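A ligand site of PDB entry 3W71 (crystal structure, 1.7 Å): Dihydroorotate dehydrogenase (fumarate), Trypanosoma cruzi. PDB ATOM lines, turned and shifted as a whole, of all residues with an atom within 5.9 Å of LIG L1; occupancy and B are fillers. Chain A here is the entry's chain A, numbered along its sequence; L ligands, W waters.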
ATOM      1  N   LYS A  44     -11.947 -14.666  13.324  1.00  0.00           N
ATOM      2  CA  LYS A  44     -12.401 -15.801  14.101  1.00  0.00           C
ATOM      3  C   LYS A  44     -11.549 -15.948  15.354  1.00  0.00           C
ATOM      4  O   LYS A  44     -10.330 -15.877  15.276  1.00  0.00           O
ATOM      5  CB  LYS A  44     -12.196 -17.017  13.254  1.00  0.00           C
ATOM      6  CG  LYS A  44     -12.560 -18.309  13.915  1.00  0.00           C
ATOM      7  CD  LYS A  44     -13.967 -18.524  14.427  1.00  0.00           C
ATOM      8  CE  LYS A  44     -14.107 -19.687  15.401  1.00  0.00           C
ATOM      9  NZ  LYS A  44     -15.560 -19.885  15.861  1.00  0.00           N
ATOM     10  N   SER A  45     -12.219 -16.151  16.478  1.00  0.00           N
ATOM     11  CA  SER A  45     -11.546 -16.423  17.770  1.00  0.00           C
ATOM     12  C   SER A  45     -10.580 -17.546  17.485  1.00  0.00           C
ATOM     13  O   SER A  45     -10.937 -18.591  16.946  1.00  0.00           O
ATOM     14  CB  SER A  45     -12.491 -16.795  18.856  1.00  0.00           C
ATOM     15  OG  SER A  45     -13.291 -15.711  19.204  1.00  0.00           O
ATOM     16  N   ARG A  51      -7.446 -25.764  14.715  1.00  0.00           N
ATOM     17  CA  ARG A  51      -8.489 -26.660  15.156  1.00  0.00           C
ATOM     18  C   ARG A  51      -9.457 -26.904  14.058  1.00  0.00           C
ATOM     19  O   ARG A  51      -9.863 -26.003  13.326  1.00  0.00           O
ATOM     20  CB  ARG A  51      -9.304 -26.119  16.334  1.00  0.00           C
ATOM     21  CG  ARG A  51      -8.524 -25.938  17.637  1.00  0.00           C
ATOM     22  CD  ARG A  51      -9.354 -25.244  18.657  1.00  0.00           C
ATOM     23  NE  ARG A  51     -10.644 -25.876  18.950  1.00  0.00           N
ATOM     24  CZ  ARG A  51     -10.824 -26.820  19.832  1.00  0.00           C
ATOM     25  NH1 ARG A  51      -9.772 -27.334  20.498  1.00  0.00           N
ATOM     26  NH2 ARG A  51     -12.032 -27.316  20.019  1.00  0.00           N
ATOM     27  N   ASN A  54     -15.837 -28.977  15.930  1.00  0.00           N
ATOM     28  CA  ASN A  54     -16.730 -30.124  16.184  1.00  0.00           C
ATOM     29  C   ASN A  54     -17.282 -30.803  14.939  1.00  0.00           C
ATOM     30  O   ASN A  54     -17.279 -30.270  13.857  1.00  0.00           O
ATOM     31  CB  ASN A  54     -17.906 -29.630  17.026  1.00  0.00           C
ATOM     32  CG  ASN A  54     -17.557 -29.370  18.456  1.00  0.00           C
ATOM     33  OD1 ASN A  54     -16.555 -29.889  18.995  1.00  0.00           O
ATOM     34  ND2 ASN A  54     -18.333 -28.521  19.087  1.00  0.00           N
ATOM     35  N   ASN A  68     -25.572 -22.951  17.263  1.00  0.00           N
ATOM     36  CA  ASN A  68     -24.278 -23.414  16.863  1.00  0.00           C
ATOM     37  C   ASN A  68     -23.519 -24.086  17.996  1.00  0.00           C
ATOM     38  O   ASN A  68     -23.524 -23.627  19.154  1.00  0.00           O
ATOM     39  CB  ASN A  68     -23.399 -22.303  16.194  1.00  0.00           C
ATOM     40  CG  ASN A  68     -22.576 -21.549  17.180  1.00  0.00           C
ATOM     41  OD1 ASN A  68     -21.462 -21.971  17.562  1.00  0.00           O
ATOM     42  ND2 ASN A  68     -23.025 -20.404  17.530  1.00  0.00           N
ATOM     43  N   SER A  69     -22.714 -25.061  17.640  1.00  0.00           N
ATOM     44  CA  SER A  69     -21.666 -25.593  18.477  1.00  0.00           C
ATOM     45  C   SER A  69     -20.471 -25.870  17.553  1.00  0.00           C
ATOM     46  O   SER A  69     -20.027 -27.015  17.353  1.00  0.00           O
ATOM     47  CB  SER A  69     -22.142 -26.838  19.262  1.00  0.00           C
ATOM     48  OG  SER A  69     -21.066 -27.258  20.113  1.00  0.00           O
ATOM     49  N   MET A  70     -19.862 -24.787  17.090  1.00  0.00           N
ATOM     50  CA  MET A  70     -18.789 -24.929  16.102  1.00  0.00           C
ATOM     51  C   MET A  70     -17.551 -25.603  16.745  1.00  0.00           C
ATOM     52  O   MET A  70     -16.821 -26.375  16.086  1.00  0.00           O
ATOM     53  CB  MET A  70     -18.406 -23.579  15.623  1.00  0.00           C
ATOM     54  CG  MET A  70     -19.414 -22.725  14.953  1.00  0.00           C
ATOM     55  SD  MET A  70     -20.275 -23.472  13.589  1.00  0.00           S
ATOM     56  CE  MET A  70     -19.058 -23.502  12.364  1.00  0.00           C
ATOM     57  N   GLY A  71     -17.292 -25.323  18.032  1.00  0.00           N
ATOM     58  CA  GLY A  71     -16.071 -25.909  18.629  1.00  0.00           C
ATOM     59  C   GLY A  71     -14.757 -25.208  18.284  1.00  0.00           C
ATOM     60  O   GLY A  71     -13.701 -25.866  18.245  1.00  0.00           O
ATOM     61  N   LEU A  72     -14.806 -23.909  18.007  1.00  0.00           N
ATOM     62  CA  LEU A  72     -13.649 -23.108  17.691  1.00  0.00           C
ATOM     63  C   LEU A  72     -12.778 -23.682  16.578  1.00  0.00           C
ATOM     64  O   LEU A  72     -11.509 -23.676  16.614  1.00  0.00           O
ATOM     65  CB  LEU A  72     -12.806 -22.948  18.995  1.00  0.00           C
ATOM     66  CG  LEU A  72     -12.162 -21.687  19.511  1.00  0.00           C
ATOM     67  CD1 LEU A  72     -12.864 -20.361  19.284  1.00  0.00           C
ATOM     68  CD2 LEU A  72     -11.817 -21.963  21.028  1.00  0.00           C
ATOM     69  N   PRO A  73     -13.399 -24.012  15.458  1.00  0.00           N
ATOM     70  CA  PRO A  73     -12.551 -24.294  14.281  1.00  0.00           C
ATOM     71  C   PRO A  73     -11.794 -23.037  13.858  1.00  0.00           C
ATOM     72  O   PRO A  73     -12.400 -21.959  13.763  1.00  0.00           O
ATOM     73  CB  PRO A  73     -13.577 -24.666  13.210  1.00  0.00           C
ATOM     74  CG  PRO A  73     -14.825 -24.072  13.604  1.00  0.00           C
ATOM     75  CD  PRO A  73     -14.785 -23.695  15.083  1.00  0.00           C
ATOM     76  N   SER A 100      -9.244 -16.778  21.733  1.00  0.00           N
ATOM     77  CA  SER A 100      -9.952 -17.603  22.681  1.00  0.00           C
ATOM     78  C   SER A 100      -9.162 -18.837  23.074  1.00  0.00           C
ATOM     79  O   SER A 100      -9.612 -19.999  22.910  1.00  0.00           O
ATOM     80  CB  SER A 100     -11.329 -17.957  22.090  1.00  0.00           C
ATOM     81  OG  SER A 100     -11.994 -18.890  22.927  1.00  0.00           O
ATOM     82  N   LEU A 102      -7.611 -21.790  25.423  1.00  0.00           N
ATOM     83  CA  LEU A 102      -8.304 -22.757  26.286  1.00  0.00           C
ATOM     84  C   LEU A 102      -7.747 -22.773  27.742  1.00  0.00           C
ATOM     85  O   LEU A 102      -8.222 -23.529  28.605  1.00  0.00           O
ATOM     86  CB  LEU A 102      -8.230 -24.149  25.668  1.00  0.00           C
ATOM     87  CG  LEU A 102      -8.648 -24.284  24.186  1.00  0.00           C
ATOM     88  CD1 LEU A 102      -8.670 -25.759  23.804  1.00  0.00           C
ATOM     89  CD2 LEU A 102      -9.956 -23.655  23.878  1.00  0.00           C
ATOM     90  N   ASN A 128     -12.019 -13.183  23.996  1.00  0.00           N
ATOM     91  CA  ASN A 128     -13.261 -13.860  24.185  1.00  0.00           C
ATOM     92  C   ASN A 128     -13.291 -14.578  25.546  1.00  0.00           C
ATOM     93  O   ASN A 128     -12.590 -15.607  25.731  1.00  0.00           O
ATOM     94  CB  ASN A 128     -13.403 -14.915  23.079  1.00  0.00           C
ATOM     95  CG  ASN A 128     -14.745 -15.587  23.092  1.00  0.00           C
ATOM     96  OD1 ASN A 128     -15.549 -15.398  23.927  1.00  0.00           O
ATOM     97  ND2 ASN A 128     -14.919 -16.482  22.087  1.00  0.00           N
ATOM     98  N   SER A 130     -16.087 -15.869  26.778  1.00  0.00           N
ATOM     99  CA  SER A 130     -17.255 -16.735  26.832  1.00  0.00           C
ATOM    100  C   SER A 130     -16.886 -17.861  26.159  1.00  0.00           C
ATOM    101  O   SER A 130     -17.346 -18.094  25.069  1.00  0.00           O
ATOM    102  CB  SER A 130     -18.518 -16.253  26.097  1.00  0.00           C
ATOM    103  OG  SER A 130     -19.424 -17.321  26.129  1.00  0.00           O
ATOM    104  N   CYS A 131     -16.094 -18.636  26.857  1.00  0.00           N
ATOM    105  CA  CYS A 131     -15.274 -19.581  26.349  1.00  0.00           C
ATOM    106  C   CYS A 131     -14.829 -20.624  27.483  1.00  0.00           C
ATOM    107  O   CYS A 131     -14.469 -20.226  28.611  1.00  0.00           O
ATOM    108  CB  CYS A 131     -13.987 -18.745  26.122  1.00  0.00           C
ATOM    109  SG  CYS A 131     -12.566 -19.744  25.632  1.00  0.00           S
ATOM    110  N   PRO A 132     -14.797 -21.929  27.155  1.00  0.00           N
ATOM    111  CA  PRO A 132     -14.049 -22.955  27.886  1.00  0.00           C
ATOM    112  C   PRO A 132     -12.905 -22.710  28.877  1.00  0.00           C
ATOM    113  O   PRO A 132     -11.798 -22.298  28.559  1.00  0.00           O
ATOM    114  CB  PRO A 132     -13.579 -23.841  26.722  1.00  0.00           C
ATOM    115  CG  PRO A 132     -14.884 -23.940  25.932  1.00  0.00           C
ATOM    116  CD  PRO A 132     -15.607 -22.584  26.105  1.00  0.00           C
ATOM    117  N   LYS A 165     -15.058  -9.821  24.911  1.00  0.00           N
ATOM    118  CA  LYS A 165     -16.390 -10.316  24.422  1.00  0.00           C
ATOM    119  C   LYS A 165     -17.005 -11.112  25.594  1.00  0.00           C
ATOM    120  O   LYS A 165     -16.433 -12.027  26.148  1.00  0.00           O
ATOM    121  CB  LYS A 165     -16.168 -11.225  23.252  1.00  0.00           C
ATOM    122  CG  LYS A 165     -17.422 -11.939  22.668  1.00  0.00           C
ATOM    123  CD  LYS A 165     -18.237 -10.945  21.879  1.00  0.00           C
ATOM    124  CE  LYS A 165     -19.272 -11.696  21.088  1.00  0.00           C
ATOM    125  NZ  LYS A 165     -18.774 -12.344  19.887  1.00  0.00           N
ATOM    126  N   ASN A 195     -22.061 -12.364  23.414  1.00  0.00           N
ATOM    127  CA  ASN A 195     -21.934 -13.714  22.768  1.00  0.00           C
ATOM    128  C   ASN A 195     -23.290 -14.465  22.703  1.00  0.00           C
ATOM    129  O   ASN A 195     -24.332 -13.990  23.203  1.00  0.00           O
ATOM    130  CB  ASN A 195     -20.836 -14.509  23.510  1.00  0.00           C
ATOM    131  CG  ASN A 195     -20.060 -15.435  22.606  1.00  0.00           C
ATOM    132  OD1 ASN A 195     -20.609 -16.122  21.775  1.00  0.00           O
ATOM    133  ND2 ASN A 195     -18.716 -15.350  22.691  1.00  0.00           N
ATOM    134  N   SER A 196     -23.293 -15.662  22.113  1.00  0.00           N
ATOM    135  CA  SER A 196     -24.528 -16.459  22.029  1.00  0.00           C
ATOM    136  C   SER A 196     -25.149 -16.731  23.366  1.00  0.00           C
ATOM    137  O   SER A 196     -24.432 -16.838  24.399  1.00  0.00           O
ATOM    138  CB  SER A 196     -24.212 -17.690  21.152  1.00  0.00           C
ATOM    139  OG  SER A 196     -23.128 -18.322  21.688  1.00  0.00           O
ATOM    140  N   PRO A 214     -23.110 -31.936  17.750  1.00  0.00           N
ATOM    141  CA  PRO A 214     -22.370 -31.925  19.036  1.00  0.00           C
ATOM    142  C   PRO A 214     -23.280 -31.780  20.243  1.00  0.00           C
ATOM    143  O   PRO A 214     -24.390 -31.241  20.113  1.00  0.00           O
ATOM    144  CB  PRO A 214     -21.508 -30.679  18.896  1.00  0.00           C
ATOM    145  CG  PRO A 214     -21.351 -30.488  17.434  1.00  0.00           C
ATOM    146  CD  PRO A 214     -22.695 -30.804  16.913  1.00  0.00           C
ATOM    147  N   LYS A 215     -22.840 -32.254  21.412  1.00  0.00           N
ATOM    148  CA  LYS A 215     -23.482 -31.985  22.703  1.00  0.00           C
ATOM    149  C   LYS A 215     -24.976 -32.308  22.727  1.00  0.00           C
ATOM    150  O   LYS A 215     -25.779 -31.604  23.325  1.00  0.00           O
ATOM    151  CB  LYS A 215     -23.223 -30.530  23.128  1.00  0.00           C
ATOM    152  CG  LYS A 215     -21.770 -30.203  23.379  1.00  0.00           C
ATOM    153  CD  LYS A 215     -21.602 -28.711  23.714  1.00  0.00           C
ATOM    154  CE  LYS A 215     -22.642 -28.086  24.633  1.00  0.00           C
ATOM    155  NZ  LYS A 215     -22.285 -26.698  25.038  1.00  0.00           N
ATOM    156  N   GLY A 220     -25.156 -22.662  21.184  1.00  0.00           N
ATOM    157  CA  GLY A 220     -25.444 -21.254  21.522  1.00  0.00           C
ATOM    158  C   GLY A 220     -26.425 -20.663  20.502  1.00  0.00           C
ATOM    159  O   GLY A 220     -26.357 -20.931  19.324  1.00  0.00           O
HETATM  160  O1  LIG L   1     -18.464 -22.732  18.868  1.00  0.00           O
HETATM  161  C1  LIG L   1     -17.734 -21.738  18.722  1.00  0.00           C
HETATM  162  O2  LIG L   1     -16.629 -21.702  18.078  1.00  0.00           O
HETATM  163  C2  LIG L   1     -18.213 -20.500  19.406  1.00  0.00           C
HETATM  164  N1  LIG L   1     -19.607 -20.232  19.139  1.00  0.00           N
HETATM  165  C3  LIG L   1     -20.239 -19.148  19.715  1.00  0.00           C
HETATM  166  O3  LIG L   1     -21.466 -18.952  19.528  1.00  0.00           O
HETATM  167  N2  LIG L   1     -19.428 -18.306  20.431  1.00  0.00           N
HETATM  168  C4  LIG L   1     -18.094 -18.540  20.783  1.00  0.00           C
HETATM  169  O4  LIG L   1     -17.480 -17.706  21.498  1.00  0.00           O
HETATM  170  C5  LIG L   1     -17.467 -19.669  20.177  1.00  0.00           C
HETATM  171  C6  LIG L   1     -16.099 -19.912  20.541  1.00  0.00           C
HETATM  172  C7  LIG L   1     -15.967 -20.326  22.019  1.00  0.00           C
HETATM  173  C8  LIG L   1     -16.226 -21.739  22.155  1.00  0.00           C
HETATM  174  C9  LIG L   1     -15.235 -22.677  22.293  1.00  0.00           C
HETATM  175  C10 LIG L   1     -15.522 -24.091  22.362  1.00  0.00           C
HETATM  176  C11 LIG L   1     -17.539 -22.303  22.132  1.00  0.00           C
HETATM  177  C12 LIG L   1     -17.842 -23.684  22.182  1.00  0.00           C
HETATM  178  C13 LIG L   1     -16.817 -24.650  22.315  1.00  0.00           C
HETATM  179  C14 LIG L   1     -17.121 -26.059  22.397  1.00  0.00           C
HETATM  180  C15 LIG L   1     -16.096 -27.028  22.284  1.00  0.00           C
HETATM  181  C16 LIG L   1     -16.407 -28.394  22.366  1.00  0.00           C
HETATM  182  C17 LIG L   1     -17.735 -28.798  22.519  1.00  0.00           C
HETATM  183  C18 LIG L   1     -18.770 -27.900  22.551  1.00  0.00           C
HETATM  184  C19 LIG L   1     -18.466 -26.528  22.512  1.00  0.00           C
HETATM  185  N1  LG2 L   2     -18.265 -15.374  19.193  1.00  0.00           N
HETATM  186  C1  LG2 L   2     -16.950 -15.196  19.463  1.00  0.00           C
HETATM  187  O1  LG2 L   2     -16.621 -14.312  20.273  1.00  0.00           O
HETATM  188  N2  LG2 L   2     -15.980 -15.962  18.897  1.00  0.00           N
HETATM  189  C2  LG2 L   2     -16.265 -16.884  17.914  1.00  0.00           C
HETATM  190  O2  LG2 L   2     -15.346 -17.557  17.315  1.00  0.00           O
HETATM  191  C3  LG2 L   2     -17.641 -17.128  17.539  1.00  0.00           C
HETATM  192  N3  LG2 L   2     -18.019 -18.058  16.631  1.00  0.00           N
HETATM  193  C4  LG2 L   2     -19.302 -18.068  16.125  1.00  0.00           C
HETATM  194  C5  LG2 L   2     -19.614 -18.857  15.013  1.00  0.00           C
HETATM  195  C6  LG2 L   2     -20.933 -18.931  14.618  1.00  0.00           C
HETATM  196  C7  LG2 L   2     -21.271 -19.824  13.444  1.00  0.00           C
HETATM  197  C8  LG2 L   2     -21.893 -18.081  15.230  1.00  0.00           C
HETATM  198  C9  LG2 L   2     -23.292 -18.101  14.777  1.00  0.00           C
HETATM  199  C10 LG2 L   2     -21.586 -17.285  16.309  1.00  0.00           C
HETATM  200  C11 LG2 L   2     -20.304 -17.257  16.794  1.00  0.00           C
HETATM  201  N4  LG2 L   2     -19.946 -16.406  17.886  1.00  0.00           N
HETATM  202  C12 LG2 L   2     -18.649 -16.265  18.235  1.00  0.00           C
HETATM  203  C13 LG2 L   2     -20.940 -15.556  18.496  1.00  0.00           C
HETATM  204  C14 LG2 L   2     -21.197 -14.305  17.677  1.00  0.00           C
HETATM  205  O3  LG2 L   2     -20.051 -13.535  17.596  1.00  0.00           O
HETATM  206  C15 LG2 L   2     -22.312 -13.492  18.291  1.00  0.00           C
HETATM  207  O4  LG2 L   2     -21.887 -13.080  19.610  1.00  0.00           O
HETATM  208  C16 LG2 L   2     -23.644 -14.283  18.435  1.00  0.00           C
HETATM  209  O5  LG2 L   2     -23.914 -15.041  17.238  1.00  0.00           O
HETATM  210  C17 LG2 L   2     -24.832 -13.291  18.566  1.00  0.00           C
HETATM  211  O6  LG2 L   2     -25.006 -12.351  17.534  1.00  0.00           O
HETATM  212  P1  LG2 L   2     -26.176 -12.561  16.434  1.00  0.00           P
HETATM  213  O7  LG2 L   2     -25.995 -11.446  15.448  1.00  0.00           O
HETATM  214  O8  LG2 L   2     -27.473 -12.626  17.144  1.00  0.00           O
HETATM  215  O9  LG2 L   2     -25.889 -13.930  15.821  1.00  0.00           O
HETATM  216  O   HOH W   1     -13.880 -26.838  24.441  1.00  0.00           O
HETATM  217  O   HOH W   2     -20.741 -22.743  20.546  1.00  0.00           O
HETATM  218  O   HOH W   3     -18.135 -26.808  25.721  1.00  0.00           O
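The side-chain amide nitrogen of Asn 128 is in hydrogen-bond range of an oxygen (O4) of LIG L1, at 2.9 Å. An oxygen (O1) of LIG L1 lies within hydrogen-bond range of the backbone NH of Gly 71, at 3.0 Å. NZ of Lys 165 sits at hydrogen-bond distance from O3 of LG2 L2. The side-chain hydroxyl (OG) of Ser 196 lies within hydrogen-bond range of an oxygen (O3) of LIG L1, at 2.8 Å. The side-chain amino group of Lys 44 sits at hydrogen-bond distance from an oxygen (O2) of LG2 L2 (2.8 Å). ND2 of Asn 195 is in hydrogen-bond range of O1 of LG2 L2. The side-chain amide nitrogen of Asn 128 lies within hydrogen-bond range of an oxygen (O1) of LG2 L2 (3.3 Å). The side-chain hydroxyl (OG) of Ser 45 lies within hydrogen-bond range of a nitrogen (N2) of LG2 L2. O1 of LIG L1 lies within hydrogen-bond range of N of Met 70. The side-chain amino group (NZ) of Lys 44 is in salt-bridge range of an oxygen (O2) of LIG L1 (3.1 Å). The side-chain amide nitrogen (ND2) of Asn 68 sits at hydrogen-bond distance from an oxygen (O3) of LIG L1 (2.9 Å). N2 of LIG L1 sits at hydrogen-bond distance from OD1 of Asn 195 (2.8 Å). N of Leu 72 is in hydrogen-bond range of O2 of LIG L1 (2.9 Å).
A nitrogen (N2) of LIG L1 sits close to a nitrogen (N1) of LG2 L2, at 3.4 Å.
O of Gly 71 sits at hydrogen-bond distance from NH2 of Arg 51, at 2.8 Å. The side-chain amide nitrogen (ND2) of Asn 128 lies within hydrogen-bond range of the side-chain hydroxyl (OG) of Ser 45. The side-chain amide oxygen (OD1) of Asn 128 lies within hydrogen-bond range of the backbone NH (N) of Ser 130, 2.9 Å away. ND2 of Asn 54 sits at hydrogen-bond distance from O of Ser 69, 2.9 Å away. OD1 of Asn 68 lies within hydrogen-bond range of N of Met 70. O of Leu 72 sits close to NE of Arg 51 (3.3 Å). OD1 of Asn 128 sits at hydrogen-bond distance from ND2 of Asn 195 (3.4 Å). The side-chain hydroxyl (OG) of Ser 196 is in hydrogen-bond range of the side-chain amide oxygen (OD1) of Asn 195 (3.3 Å).
ND2 of Asn 54 touches C17 of LIG L1, 3.5 Å away. Ser 69 touches LIG L1 (OG to C18, 3.4 Å). O of Ser 130 touches O4 of LIG L1, 3.6 Å away. CG of Pro 132 touches C10 of LIG L1, 3.6 Å away. Lys 215 touches LIG L1. 13 residues have an atom within 4 Å of LIG L1: Lys 44, Asn 54, Asn 68, Ser 69, Met 70, Gly 71, Leu 72, Asn 128, Ser 130, Pro 132, Asn 195, Ser 196 and Lys 215. The nearest printed residue that does not touch LIG L1 is Pro 73 (4.04 Å).
Water W2 bridges O1 of LIG L1 (2.8 Å) and OD1 of Asn 68 (3.2 Å).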
